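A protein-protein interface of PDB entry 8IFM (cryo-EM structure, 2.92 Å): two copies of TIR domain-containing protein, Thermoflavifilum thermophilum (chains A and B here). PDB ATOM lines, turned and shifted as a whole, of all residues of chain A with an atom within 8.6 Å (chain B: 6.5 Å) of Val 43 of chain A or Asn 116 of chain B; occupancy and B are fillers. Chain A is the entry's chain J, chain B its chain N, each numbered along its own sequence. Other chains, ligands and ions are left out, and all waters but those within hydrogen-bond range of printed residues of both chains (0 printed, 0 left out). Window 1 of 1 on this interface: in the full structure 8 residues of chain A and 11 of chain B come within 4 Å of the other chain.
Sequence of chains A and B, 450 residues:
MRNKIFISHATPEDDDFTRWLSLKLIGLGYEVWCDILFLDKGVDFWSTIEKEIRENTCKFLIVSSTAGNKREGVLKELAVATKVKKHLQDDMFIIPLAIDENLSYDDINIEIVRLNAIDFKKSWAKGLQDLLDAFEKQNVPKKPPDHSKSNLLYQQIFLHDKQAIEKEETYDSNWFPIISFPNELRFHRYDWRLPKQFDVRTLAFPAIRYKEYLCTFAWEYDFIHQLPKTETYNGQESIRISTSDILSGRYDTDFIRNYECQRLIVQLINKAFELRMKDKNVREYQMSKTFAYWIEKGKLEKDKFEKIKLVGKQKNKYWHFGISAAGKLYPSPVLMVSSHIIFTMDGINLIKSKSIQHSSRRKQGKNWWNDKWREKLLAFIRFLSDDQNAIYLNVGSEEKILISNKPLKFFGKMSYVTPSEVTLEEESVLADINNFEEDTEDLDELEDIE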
ATOM      1  N   TRP A  33      13.284  -1.381   1.219  1.00  0.00           N
ATOM      2  CA  TRP A  33      13.156  -2.775   0.814  1.00  0.00           C
ATOM      3  C   TRP A  33      12.051  -3.415   1.637  1.00  0.00           C
ATOM      4  O   TRP A  33      12.159  -3.493   2.865  1.00  0.00           O
ATOM      5  CB  TRP A  33      14.466  -3.543   1.000  1.00  0.00           C
ATOM      6  CG  TRP A  33      14.525  -4.786   0.174  1.00  0.00           C
ATOM      7  CD1 TRP A  33      14.971  -4.896  -1.110  1.00  0.00           C
ATOM      8  CD2 TRP A  33      14.076  -6.092   0.556  1.00  0.00           C
ATOM      9  NE1 TRP A  33      14.854  -6.194  -1.541  1.00  0.00           N
ATOM     10  CE2 TRP A  33      14.304  -6.947  -0.537  1.00  0.00           C
ATOM     11  CE3 TRP A  33      13.514  -6.620   1.720  1.00  0.00           C
ATOM     12  CZ2 TRP A  33      13.990  -8.303  -0.501  1.00  0.00           C
ATOM     13  CZ3 TRP A  33      13.205  -7.967   1.755  1.00  0.00           C
ATOM     14  CH2 TRP A  33      13.443  -8.792   0.652  1.00  0.00           C
ATOM     15  N   ASP A  35       9.269  -6.868   1.767  1.00  0.00           N
ATOM     16  CA  ASP A  35       9.110  -8.219   1.234  1.00  0.00           C
ATOM     17  C   ASP A  35       7.854  -8.357   0.380  1.00  0.00           C
ATOM     18  O   ASP A  35       7.814  -9.197  -0.525  1.00  0.00           O
ATOM     19  CB  ASP A  35       9.115  -9.244   2.373  1.00  0.00           C
ATOM     20  CG  ASP A  35       7.767  -9.377   3.062  1.00  0.00           C
ATOM     21  OD1 ASP A  35       6.986  -8.405   3.072  1.00  0.00           O
ATOM     22  OD2 ASP A  35       7.488 -10.470   3.601  1.00  0.00           O
ATOM     23  N   ILE A  36       6.816  -7.558   0.652  1.00  0.00           N
ATOM     24  CA  ILE A  36       5.611  -7.594  -0.173  1.00  0.00           C
ATOM     25  C   ILE A  36       5.682  -6.627  -1.345  1.00  0.00           C
ATOM     26  O   ILE A  36       4.753  -6.592  -2.163  1.00  0.00           O
ATOM     27  CB  ILE A  36       4.347  -7.306   0.663  1.00  0.00           C
ATOM     28  CG1 ILE A  36       4.513  -6.015   1.462  1.00  0.00           C
ATOM     29  CG2 ILE A  36       4.042  -8.476   1.586  1.00  0.00           C
ATOM     30  CD1 ILE A  36       3.365  -5.724   2.397  1.00  0.00           C
ATOM     31  N   PHE A  38       9.330  -5.447  -2.695  1.00  0.00           N
ATOM     32  CA  PHE A  38      10.615  -5.559  -3.367  1.00  0.00           C
ATOM     33  C   PHE A  38      11.186  -6.970  -3.397  1.00  0.00           C
ATOM     34  O   PHE A  38      12.155  -7.207  -4.125  1.00  0.00           O
ATOM     35  CB  PHE A  38      11.639  -4.620  -2.713  1.00  0.00           C
ATOM     36  CG  PHE A  38      11.438  -3.171  -3.056  1.00  0.00           C
ATOM     37  CD1 PHE A  38      10.440  -2.431  -2.447  1.00  0.00           C
ATOM     38  CD2 PHE A  38      12.252  -2.550  -3.990  1.00  0.00           C
ATOM     39  CE1 PHE A  38      10.255  -1.098  -2.763  1.00  0.00           C
ATOM     40  CE2 PHE A  38      12.072  -1.218  -4.310  1.00  0.00           C
ATOM     41  CZ  PHE A  38      11.073  -0.491  -3.696  1.00  0.00           C
ATOM     42  N   LEU A  39      10.626  -7.910  -2.638  1.00  0.00           N
ATOM     43  CA  LEU A  39      11.115  -9.282  -2.684  1.00  0.00           C
ATOM     44  C   LEU A  39      10.638  -9.945  -3.969  1.00  0.00           C
ATOM     45  O   LEU A  39       9.431 -10.063  -4.206  1.00  0.00           O
ATOM     46  CB  LEU A  39      10.640 -10.067  -1.465  1.00  0.00           C
ATOM     47  CG  LEU A  39      10.854 -11.577  -1.530  1.00  0.00           C
ATOM     48  CD1 LEU A  39      12.318 -11.908  -1.309  1.00  0.00           C
ATOM     49  CD2 LEU A  39       9.981 -12.287  -0.507  1.00  0.00           C
ATOM     50  N   ASP A  40      11.585 -10.377  -4.794  1.00  0.00           N
ATOM     51  CA  ASP A  40      11.259 -10.866  -6.123  1.00  0.00           C
ATOM     52  C   ASP A  40      10.608 -12.246  -6.063  1.00  0.00           C
ATOM     53  O   ASP A  40      10.774 -13.008  -5.107  1.00  0.00           O
ATOM     54  CB  ASP A  40      12.510 -10.919  -6.995  1.00  0.00           C
ATOM     55  CG  ASP A  40      12.183 -11.026  -8.465  1.00  0.00           C
ATOM     56  OD1 ASP A  40      11.587 -10.074  -9.009  1.00  0.00           O
ATOM     57  OD2 ASP A  40      12.520 -12.060  -9.079  1.00  0.00           O
ATOM     58  N   LYS A  41       9.852 -12.554  -7.113  1.00  0.00           N
ATOM     59  CA  LYS A  41       9.231 -13.859  -7.261  1.00  0.00           C
ATOM     60  C   LYS A  41      10.217 -14.852  -7.866  1.00  0.00           C
ATOM     61  O   LYS A  41      11.086 -14.490  -8.664  1.00  0.00           O
ATOM     62  CB  LYS A  41       7.988 -13.759  -8.146  1.00  0.00           C
ATOM     63  CG  LYS A  41       6.829 -12.999  -7.520  1.00  0.00           C
ATOM     64  CD  LYS A  41       6.324 -13.687  -6.263  1.00  0.00           C
ATOM     65  CE  LYS A  41       5.791 -12.683  -5.258  1.00  0.00           C
ATOM     66  NZ  LYS A  41       4.919 -13.334  -4.243  1.00  0.00           N
ATOM     67  N   GLY A  42      10.068 -16.116  -7.482  1.00  0.00           N
ATOM     68  CA  GLY A  42      10.962 -17.150  -7.981  1.00  0.00           C
ATOM     69  C   GLY A  42      12.398 -16.976  -7.539  1.00  0.00           C
ATOM     70  O   GLY A  42      13.323 -17.164  -8.340  1.00  0.00           O
ATOM     71  N   VAL A  43      12.605 -16.619  -6.274  1.00  0.00           N
ATOM     72  CA  VAL A  43      13.929 -16.338  -5.733  1.00  0.00           C
ATOM     73  C   VAL A  43      13.967 -16.849  -4.300  1.00  0.00           C
ATOM     74  O   VAL A  43      12.951 -16.853  -3.598  1.00  0.00           O
ATOM     75  CB  VAL A  43      14.254 -14.822  -5.807  1.00  0.00           C
ATOM     76  CG1 VAL A  43      15.357 -14.430  -4.837  1.00  0.00           C
ATOM     77  CG2 VAL A  43      14.640 -14.433  -7.221  1.00  0.00           C
ATOM     78  N   ASP A  44      15.143 -17.314  -3.873  1.00  0.00           N
ATOM     79  CA  ASP A  44      15.331 -17.658  -2.470  1.00  0.00           C
ATOM     80  C   ASP A  44      15.078 -16.423  -1.618  1.00  0.00           C
ATOM     81  O   ASP A  44      15.873 -15.477  -1.629  1.00  0.00           O
ATOM     82  CB  ASP A  44      16.738 -18.206  -2.228  1.00  0.00           C
ATOM     83  CG  ASP A  44      16.851 -18.968  -0.923  1.00  0.00           C
ATOM     84  OD1 ASP A  44      15.838 -19.075  -0.201  1.00  0.00           O
ATOM     85  OD2 ASP A  44      17.954 -19.469  -0.620  1.00  0.00           O
ATOM     86  N   PHE A  45      13.965 -16.423  -0.882  1.00  0.00           N
ATOM     87  CA  PHE A  45      13.560 -15.214  -0.176  1.00  0.00           C
ATOM     88  C   PHE A  45      14.417 -14.977   1.060  1.00  0.00           C
ATOM     89  O   PHE A  45      14.834 -13.845   1.315  1.00  0.00           O
ATOM     90  CB  PHE A  45      12.072 -15.282   0.185  1.00  0.00           C
ATOM     91  CG  PHE A  45      11.679 -16.494   0.986  1.00  0.00           C
ATOM     92  CD1 PHE A  45      11.503 -17.726   0.379  1.00  0.00           C
ATOM     93  CD2 PHE A  45      11.446 -16.389   2.346  1.00  0.00           C
ATOM     94  CE1 PHE A  45      11.130 -18.832   1.118  1.00  0.00           C
ATOM     95  CE2 PHE A  45      11.070 -17.490   3.088  1.00  0.00           C
ATOM     96  CZ  PHE A  45      10.912 -18.713   2.475  1.00  0.00           C
ATOM     97  N   TRP A  46      14.710 -16.030   1.824  1.00  0.00           N
ATOM     98  CA  TRP A  46      15.478 -15.862   3.055  1.00  0.00           C
ATOM     99  C   TRP A  46      16.919 -15.452   2.769  1.00  0.00           C
ATOM    100  O   TRP A  46      17.488 -14.618   3.485  1.00  0.00           O
ATOM    101  CB  TRP A  46      15.412 -17.148   3.875  1.00  0.00           C
ATOM    102  CG  TRP A  46      14.290 -17.135   4.863  1.00  0.00           C
ATOM    103  CD1 TRP A  46      13.804 -16.050   5.531  1.00  0.00           C
ATOM    104  CD2 TRP A  46      13.464 -18.242   5.244  1.00  0.00           C
ATOM    105  NE1 TRP A  46      12.755 -16.418   6.337  1.00  0.00           N
ATOM    106  CE2 TRP A  46      12.520 -17.758   6.173  1.00  0.00           C
ATOM    107  CE3 TRP A  46      13.437 -19.596   4.900  1.00  0.00           C
ATOM    108  CZ2 TRP A  46      11.564 -18.580   6.763  1.00  0.00           C
ATOM    109  CZ3 TRP A  46      12.482 -20.409   5.484  1.00  0.00           C
ATOM    110  CH2 TRP A  46      11.562 -19.900   6.409  1.00  0.00           C
ATOM    111  N   SER A  47      17.524 -16.016   1.720  1.00  0.00           N
ATOM    112  CA  SER A  47      18.876 -15.611   1.347  1.00  0.00           C
ATOM    113  C   SER A  47      18.922 -14.143   0.943  1.00  0.00           C
ATOM    114  O   SER A  47      19.840 -13.411   1.334  1.00  0.00           O
ATOM    115  CB  SER A  47      19.394 -16.495   0.212  1.00  0.00           C
ATOM    116  OG  SER A  47      20.346 -15.802  -0.575  1.00  0.00           O
ATOM    117  N   THR A  48      17.935 -13.690   0.166  1.00  0.00           N
ATOM    118  CA  THR A  48      17.898 -12.286  -0.230  1.00  0.00           C
ATOM    119  C   THR A  48      17.613 -11.376   0.957  1.00  0.00           C
ATOM    120  O   THR A  48      18.151 -10.264   1.026  1.00  0.00           O
ATOM    121  CB  THR A  48      16.856 -12.075  -1.328  1.00  0.00           C
ATOM    122  OG1 THR A  48      16.986 -13.107  -2.312  1.00  0.00           O
ATOM    123  CG2 THR A  48      17.054 -10.722  -1.997  1.00  0.00           C
ATOM    124  N   ILE A  49      16.782 -11.826   1.902  1.00  0.00           N
ATOM    125  CA  ILE A  49      16.559 -11.050   3.118  1.00  0.00           C
ATOM    126  C   ILE A  49      17.860 -10.895   3.891  1.00  0.00           C
ATOM    127  O   ILE A  49      18.174  -9.806   4.379  1.00  0.00           O
ATOM    128  CB  ILE A  49      15.455 -11.686   3.985  1.00  0.00           C
ATOM    129  CG1 ILE A  49      14.112 -11.676   3.253  1.00  0.00           C
ATOM    130  CG2 ILE A  49      15.322 -10.956   5.313  1.00  0.00           C
ATOM    131  CD1 ILE A  49      13.046 -12.510   3.933  1.00  0.00           C
ATOM    132  N   ASP B  91      19.990 -16.014  -9.784  1.00  0.00           N
ATOM    133  CA  ASP B  91      18.948 -16.545  -8.912  1.00  0.00           C
ATOM    134  C   ASP B  91      17.545 -16.278  -9.440  1.00  0.00           C
ATOM    135  O   ASP B  91      16.587 -16.871  -8.932  1.00  0.00           O
ATOM    136  CB  ASP B  91      19.084 -15.956  -7.508  1.00  0.00           C
ATOM    137  CG  ASP B  91      18.714 -16.948  -6.422  1.00  0.00           C
ATOM    138  OD1 ASP B  91      19.391 -17.993  -6.322  1.00  0.00           O
ATOM    139  OD2 ASP B  91      17.754 -16.682  -5.667  1.00  0.00           O
ATOM    140  N   MET B  92      17.400 -15.401 -10.430  1.00  0.00           N
ATOM    141  CA  MET B  92      16.091 -15.046 -10.975  1.00  0.00           C
ATOM    142  C   MET B  92      15.774 -15.884 -12.215  1.00  0.00           C
ATOM    143  O   MET B  92      15.524 -15.371 -13.303  1.00  0.00           O
ATOM    144  CB  MET B  92      16.046 -13.555 -11.293  1.00  0.00           C
ATOM    145  CG  MET B  92      15.781 -12.667 -10.090  1.00  0.00           C
ATOM    146  SD  MET B  92      16.482 -11.014 -10.255  1.00  0.00           S
ATOM    147  CE  MET B  92      17.983 -11.189  -9.294  1.00  0.00           C
ATOM    148  N   PHE B  93      15.780 -17.205 -12.033  1.00  0.00           N
ATOM    149  CA  PHE B  93      15.510 -18.125 -13.129  1.00  0.00           C
ATOM    150  C   PHE B  93      14.205 -18.887 -12.941  1.00  0.00           C
ATOM    151  O   PHE B  93      13.290 -18.762 -13.760  1.00  0.00           O
ATOM    152  CB  PHE B  93      16.667 -19.117 -13.289  1.00  0.00           C
ATOM    153  CG  PHE B  93      16.635 -19.877 -14.584  1.00  0.00           C
ATOM    154  CD1 PHE B  93      17.108 -19.303 -15.752  1.00  0.00           C
ATOM    155  CD2 PHE B  93      16.095 -21.150 -14.638  1.00  0.00           C
ATOM    156  CE1 PHE B  93      17.071 -20.001 -16.943  1.00  0.00           C
ATOM    157  CE2 PHE B  93      16.051 -21.850 -15.824  1.00  0.00           C
ATOM    158  CZ  PHE B  93      16.539 -21.274 -16.978  1.00  0.00           C
ATOM    159  N   ILE B  94      14.082 -19.655 -11.864  1.00  0.00           N
ATOM    160  CA  ILE B  94      12.992 -20.607 -11.699  1.00  0.00           C
ATOM    161  C   ILE B  94      11.907 -19.963 -10.852  1.00  0.00           C
ATOM    162  O   ILE B  94      12.194 -19.371  -9.805  1.00  0.00           O
ATOM    163  CB  ILE B  94      13.492 -21.914 -11.062  1.00  0.00           C
ATOM    164  CG1 ILE B  94      14.452 -22.627 -12.010  1.00  0.00           C
ATOM    165  CG2 ILE B  94      12.330 -22.828 -10.759  1.00  0.00           C
ATOM    166  CD1 ILE B  94      14.936 -23.956 -11.499  1.00  0.00           C
ATOM    167  N   ILE B  95      10.663 -20.067 -11.309  1.00  0.00           N
ATOM    168  CA  ILE B  95       9.521 -19.458 -10.635  1.00  0.00           C
ATOM    169  C   ILE B  95       8.455 -20.524 -10.403  1.00  0.00           C
ATOM    170  O   ILE B  95       7.891 -21.057 -11.370  1.00  0.00           O
ATOM    171  CB  ILE B  95       8.963 -18.281 -11.449  1.00  0.00           C
ATOM    172  CG1 ILE B  95      10.078 -17.282 -11.765  1.00  0.00           C
ATOM    173  CG2 ILE B  95       7.834 -17.602 -10.696  1.00  0.00           C
ATOM    174  CD1 ILE B  95       9.600 -16.001 -12.412  1.00  0.00           C
ATOM    175  N   PRO B  96       8.172 -20.894  -9.154  1.00  0.00           N
ATOM    176  CA  PRO B  96       7.048 -21.802  -8.891  1.00  0.00           C
ATOM    177  C   PRO B  96       5.719 -21.060  -8.935  1.00  0.00           C
ATOM    178  O   PRO B  96       5.583 -19.967  -8.383  1.00  0.00           O
ATOM    179  CB  PRO B  96       7.340 -22.338  -7.487  1.00  0.00           C
ATOM    180  CG  PRO B  96       8.224 -21.320  -6.871  1.00  0.00           C
ATOM    181  CD  PRO B  96       9.037 -20.726  -7.977  1.00  0.00           C
ATOM    182  N   TYR B 105       2.018 -24.483   1.367  1.00  0.00           N
ATOM    183  CA  TYR B 105       3.410 -24.143   1.111  1.00  0.00           C
ATOM    184  C   TYR B 105       4.368 -25.112   1.786  1.00  0.00           C
ATOM    185  O   TYR B 105       5.548 -25.152   1.424  1.00  0.00           O
ATOM    186  CB  TYR B 105       3.695 -22.708   1.555  1.00  0.00           C
ATOM    187  CG  TYR B 105       3.492 -21.702   0.445  1.00  0.00           C
ATOM    188  CD1 TYR B 105       2.216 -21.380   0.002  1.00  0.00           C
ATOM    189  CD2 TYR B 105       4.575 -21.086  -0.169  1.00  0.00           C
ATOM    190  CE1 TYR B 105       2.023 -20.467  -1.016  1.00  0.00           C
ATOM    191  CE2 TYR B 105       4.391 -20.171  -1.188  1.00  0.00           C
ATOM    192  CZ  TYR B 105       3.114 -19.865  -1.607  1.00  0.00           C
ATOM    193  OH  TYR B 105       2.924 -18.956  -2.622  1.00  0.00           O
ATOM    194  N   ILE B 112      12.227 -26.644  -4.900  1.00  0.00           N
ATOM    195  CA  ILE B 112      11.477 -25.421  -5.145  1.00  0.00           C
ATOM    196  C   ILE B 112      11.030 -24.796  -3.828  1.00  0.00           C
ATOM    197  O   ILE B 112      10.543 -23.660  -3.807  1.00  0.00           O
ATOM    198  CB  ILE B 112      10.283 -25.709  -6.069  1.00  0.00           C
ATOM    199  CG1 ILE B 112       9.935 -24.463  -6.867  1.00  0.00           C
ATOM    200  CG2 ILE B 112       9.089 -26.203  -5.274  1.00  0.00           C
ATOM    201  CD1 ILE B 112      11.023 -24.039  -7.798  1.00  0.00           C
ATOM    202  N   VAL B 113      11.188 -25.528  -2.720  1.00  0.00           N
ATOM    203  CA  VAL B 113      10.811 -24.989  -1.414  1.00  0.00           C
ATOM    204  C   VAL B 113      11.663 -23.778  -1.063  1.00  0.00           C
ATOM    205  O   VAL B 113      11.204 -22.861  -0.371  1.00  0.00           O
ATOM    206  CB  VAL B 113      10.904 -26.078  -0.322  1.00  0.00           C
ATOM    207  CG1 VAL B 113      12.350 -26.406   0.005  1.00  0.00           C
ATOM    208  CG2 VAL B 113      10.173 -25.639   0.930  1.00  0.00           C
ATOM    209  N   ARG B 114      12.911 -23.752  -1.530  1.00  0.00           N
ATOM    210  CA  ARG B 114      13.806 -22.639  -1.245  1.00  0.00           C
ATOM    211  C   ARG B 114      13.368 -21.356  -1.939  1.00  0.00           C
ATOM    212  O   ARG B 114      13.735 -20.267  -1.490  1.00  0.00           O
ATOM    213  CB  ARG B 114      15.228 -23.013  -1.668  1.00  0.00           C
ATOM    214  CG  ARG B 114      16.338 -22.275  -0.944  1.00  0.00           C
ATOM    215  CD  ARG B 114      16.387 -22.609   0.538  1.00  0.00           C
ATOM    216  NE  ARG B 114      17.123 -21.598   1.286  1.00  0.00           N
ATOM    217  CZ  ARG B 114      16.960 -21.349   2.579  1.00  0.00           C
ATOM    218  NH1 ARG B 114      16.091 -22.029   3.309  1.00  0.00           N
ATOM    219  NH2 ARG B 114      17.687 -20.396   3.154  1.00  0.00           N
ATOM    220  N   LEU B 115      12.582 -21.460  -3.003  1.00  0.00           N
ATOM    221  CA  LEU B 115      12.269 -20.336  -3.872  1.00  0.00           C
ATOM    222  C   LEU B 115      10.909 -19.737  -3.528  1.00  0.00           C
ATOM    223  O   LEU B 115      10.077 -20.358  -2.860  1.00  0.00           O
ATOM    224  CB  LEU B 115      12.304 -20.782  -5.336  1.00  0.00           C
ATOM    225  CG  LEU B 115      13.630 -20.558  -6.067  1.00  0.00           C
ATOM    226  CD1 LEU B 115      14.775 -21.266  -5.362  1.00  0.00           C
ATOM    227  CD2 LEU B 115      13.526 -21.045  -7.492  1.00  0.00           C
ATOM    228  N   ASN B 116      10.692 -18.511  -3.999  1.00  0.00           N
ATOM    229  CA  ASN B 116       9.472 -17.763  -3.715  1.00  0.00           C
ATOM    230  C   ASN B 116       8.420 -18.070  -4.774  1.00  0.00           C
ATOM    231  O   ASN B 116       8.632 -17.807  -5.962  1.00  0.00           O
ATOM    232  CB  ASN B 116       9.759 -16.263  -3.669  1.00  0.00           C
ATOM    233  CG  ASN B 116       8.646 -15.477  -3.009  1.00  0.00           C
ATOM    234  OD1 ASN B 116       7.731 -16.051  -2.417  1.00  0.00           O
ATOM    235  ND2 ASN B 116       8.716 -14.155  -3.108  1.00  0.00           N
ATOM    236  N   ALA B 117       7.287 -18.616  -4.343  1.00  0.00           N
ATOM    237  CA  ALA B 117       6.223 -18.972  -5.266  1.00  0.00           C
ATOM    238  C   ALA B 117       5.367 -17.757  -5.609  1.00  0.00           C
ATOM    239  O   ALA B 117       5.393 -16.728  -4.930  1.00  0.00           O
ATOM    240  CB  ALA B 117       5.348 -20.078  -4.677  1.00  0.00           C
ATOM    241  N   ILE B 118       4.597 -17.893  -6.686  1.00  0.00           N
ATOM    242  CA  ILE B 118       3.621 -16.891  -7.097  1.00  0.00           C
ATOM    243  C   ILE B 118       2.244 -17.441  -6.763  1.00  0.00           C
ATOM    244  O   ILE B 118       1.881 -18.537  -7.207  1.00  0.00           O
ATOM    245  CB  ILE B 118       3.737 -16.555  -8.590  1.00  0.00           C
ATOM    246  CG1 ILE B 118       5.070 -15.865  -8.876  1.00  0.00           C
ATOM    247  CG2 ILE B 118       2.586 -15.664  -9.019  1.00  0.00           C
ATOM    248  CD1 ILE B 118       5.124 -15.158 -10.209  1.00  0.00           C
ATOM    249  N   GLN B 138      12.512  -8.153 -14.199  1.00  0.00           N
ATOM    250  CA  GLN B 138      13.682  -8.955 -14.529  1.00  0.00           C
ATOM    251  C   GLN B 138      14.102  -8.814 -15.988  1.00  0.00           C
ATOM    252  O   GLN B 138      14.914  -9.612 -16.469  1.00  0.00           O
ATOM    253  CB  GLN B 138      13.427 -10.425 -14.195  1.00  0.00           C
ATOM    254  CG  GLN B 138      13.987 -10.835 -12.852  1.00  0.00           C
ATOM    255  CD  GLN B 138      13.051 -10.502 -11.713  1.00  0.00           C
ATOM    256  OE1 GLN B 138      11.918 -10.977 -11.666  1.00  0.00           O
ATOM    257  NE2 GLN B 138      13.516  -9.660 -10.798  1.00  0.00           N
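The backbone carbonyl oxygen of Asp 40 of chain A is in hydrogen-bond range of the side-chain amide nitrogen of Asn 116 of chain B (3.1 Å).
The side-chain carboxylate (OD1) of Asp 40 of chain A sits at hydrogen-bond distance from the side-chain amide nitrogen (NE2) of Gln 138 of chain B, at 2.7 Å.
The backbone carbonyl oxygen of Ala 117 of chain B lies close to the side-chain amino group of Lys 41 of chain A, 3.5 Å away.
The backbone NH (N) of Gly 42 of chain A lies within hydrogen-bond range of the backbone carbonyl oxygen (O) of Asn 116 of chain B, at 2.7 Å.
The backbone carbonyl oxygen of Val 43 of chain A lies within hydrogen-bond range of the backbone NH of Asn 116 of chain B, 2.8 Å away.
The side-chain carboxylate (OD2) of Asp 91 of chain B sits at hydrogen-bond distance from the backbone NH (N) of Asp 44 of chain A.
NE of Arg 114 of chain B is in salt-bridge range of OD2 of Asp 44 of chain A.
The backbone carbonyl oxygen (O) of Gly 42 of chain A lies close to the backbone carbonyl oxygen (O) of Asp 91 of chain B (3.3 Å).
The backbone carbonyl oxygen (O) of Gly 42 of chain A sits close to the backbone carbonyl oxygen (O) of Ile 94 of chain B.
The backbone carbonyl oxygen of Asp 44 of chain A is in hydrogen-bond range of the side-chain hydroxyl of Thr 48 of chain A (2.7 Å).
The side-chain sulfur (SD) of Met 92 of chain B lies within hydrogen-bond range of the side-chain amide nitrogen (NE2) of Gln 138 of chain B, 3.3 Å away.
The backbone NH (N) of Ile 118 of chain B is in hydrogen-bond range of the backbone carbonyl oxygen (O) of Pro 96 of chain B (2.9 Å).
Among the printed residues, pairs that only touch across the chains: Val 43 of chain A with Asp 91 of chain B, Leu 39 of chain A with Asn 116 of chain B, Asp 40 of chain A with Met 92 of chain B, Val 43 of chain A with Leu 115 of chain B, Val 43 of chain A with Met 92 of chain B, Lys 41 of chain A with Ile 118 of chain B, Gly 42 of chain A with Ile 95 of chain B, Lys 41 of chain A with Asn 116 of chain B, Phe 45 of chain A with Arg 114 of chain B, Trp 46 of chain A with Arg 114 of chain B and Gly 42 of chain A with Leu 115 of chain B.
Of chain B, only Asp 91 (3.4 Å), Met 92 (3.6 Å), Leu 115 (3.5 Å) and Asn 116 (2.8 Å) come within 4 Å of Val 43 of chain A.
Of chain A, only Leu 39, Asp 40, Lys 41, Gly 42 and Val 43 come within 4 Å of Asn 116 of chain B.
Of the printed residues of chain A, Ile 118 of chain B touches Lys 41 (3.6 Å).
Of the printed residues of chain B, Trp 46 of chain A touches Arg 114 (3.9 Å).
Of the printed residues of chain B, Phe 45 of chain A touches Arg 114 (3.9 Å).
The nearest residue of chain B that does not touch Val 43 of chain A is Arg 114 of chain B (4.1 Å).
The nearest residue of chain A that does not touch Asn 116 of chain B is Phe 45 of chain A (4.5 Å).
Hydrophobic or aromatic side chains of chain A that line the printed part of chain B: Leu 39, Val 43, Phe 45 and Trp 46.
Of the 15 printed residues of chain B, 10 touch a printed residue of chain A.
Printed residues of chain B that touch a printed residue of chain A: Asp 91, Met 92, Ile 94, Ile 95, Arg 114, Leu 115, Asn 116, Ala 117, Ile 118 and Gln 138.
Along chain B the printed residues that touch a printed residue of chain A span positions 91 to 138.
Among the printed residues, Asp or Glu carboxylates within 4 Å of a Lys or Arg side-chain nitrogen of the other chain: Asp 44 of chain A with Arg 114 of chain B.
No position is printed for both chains.
Of the 20 pairs that touch across the chains among the printed residues, none has its exchanged pair printed and touching as well.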
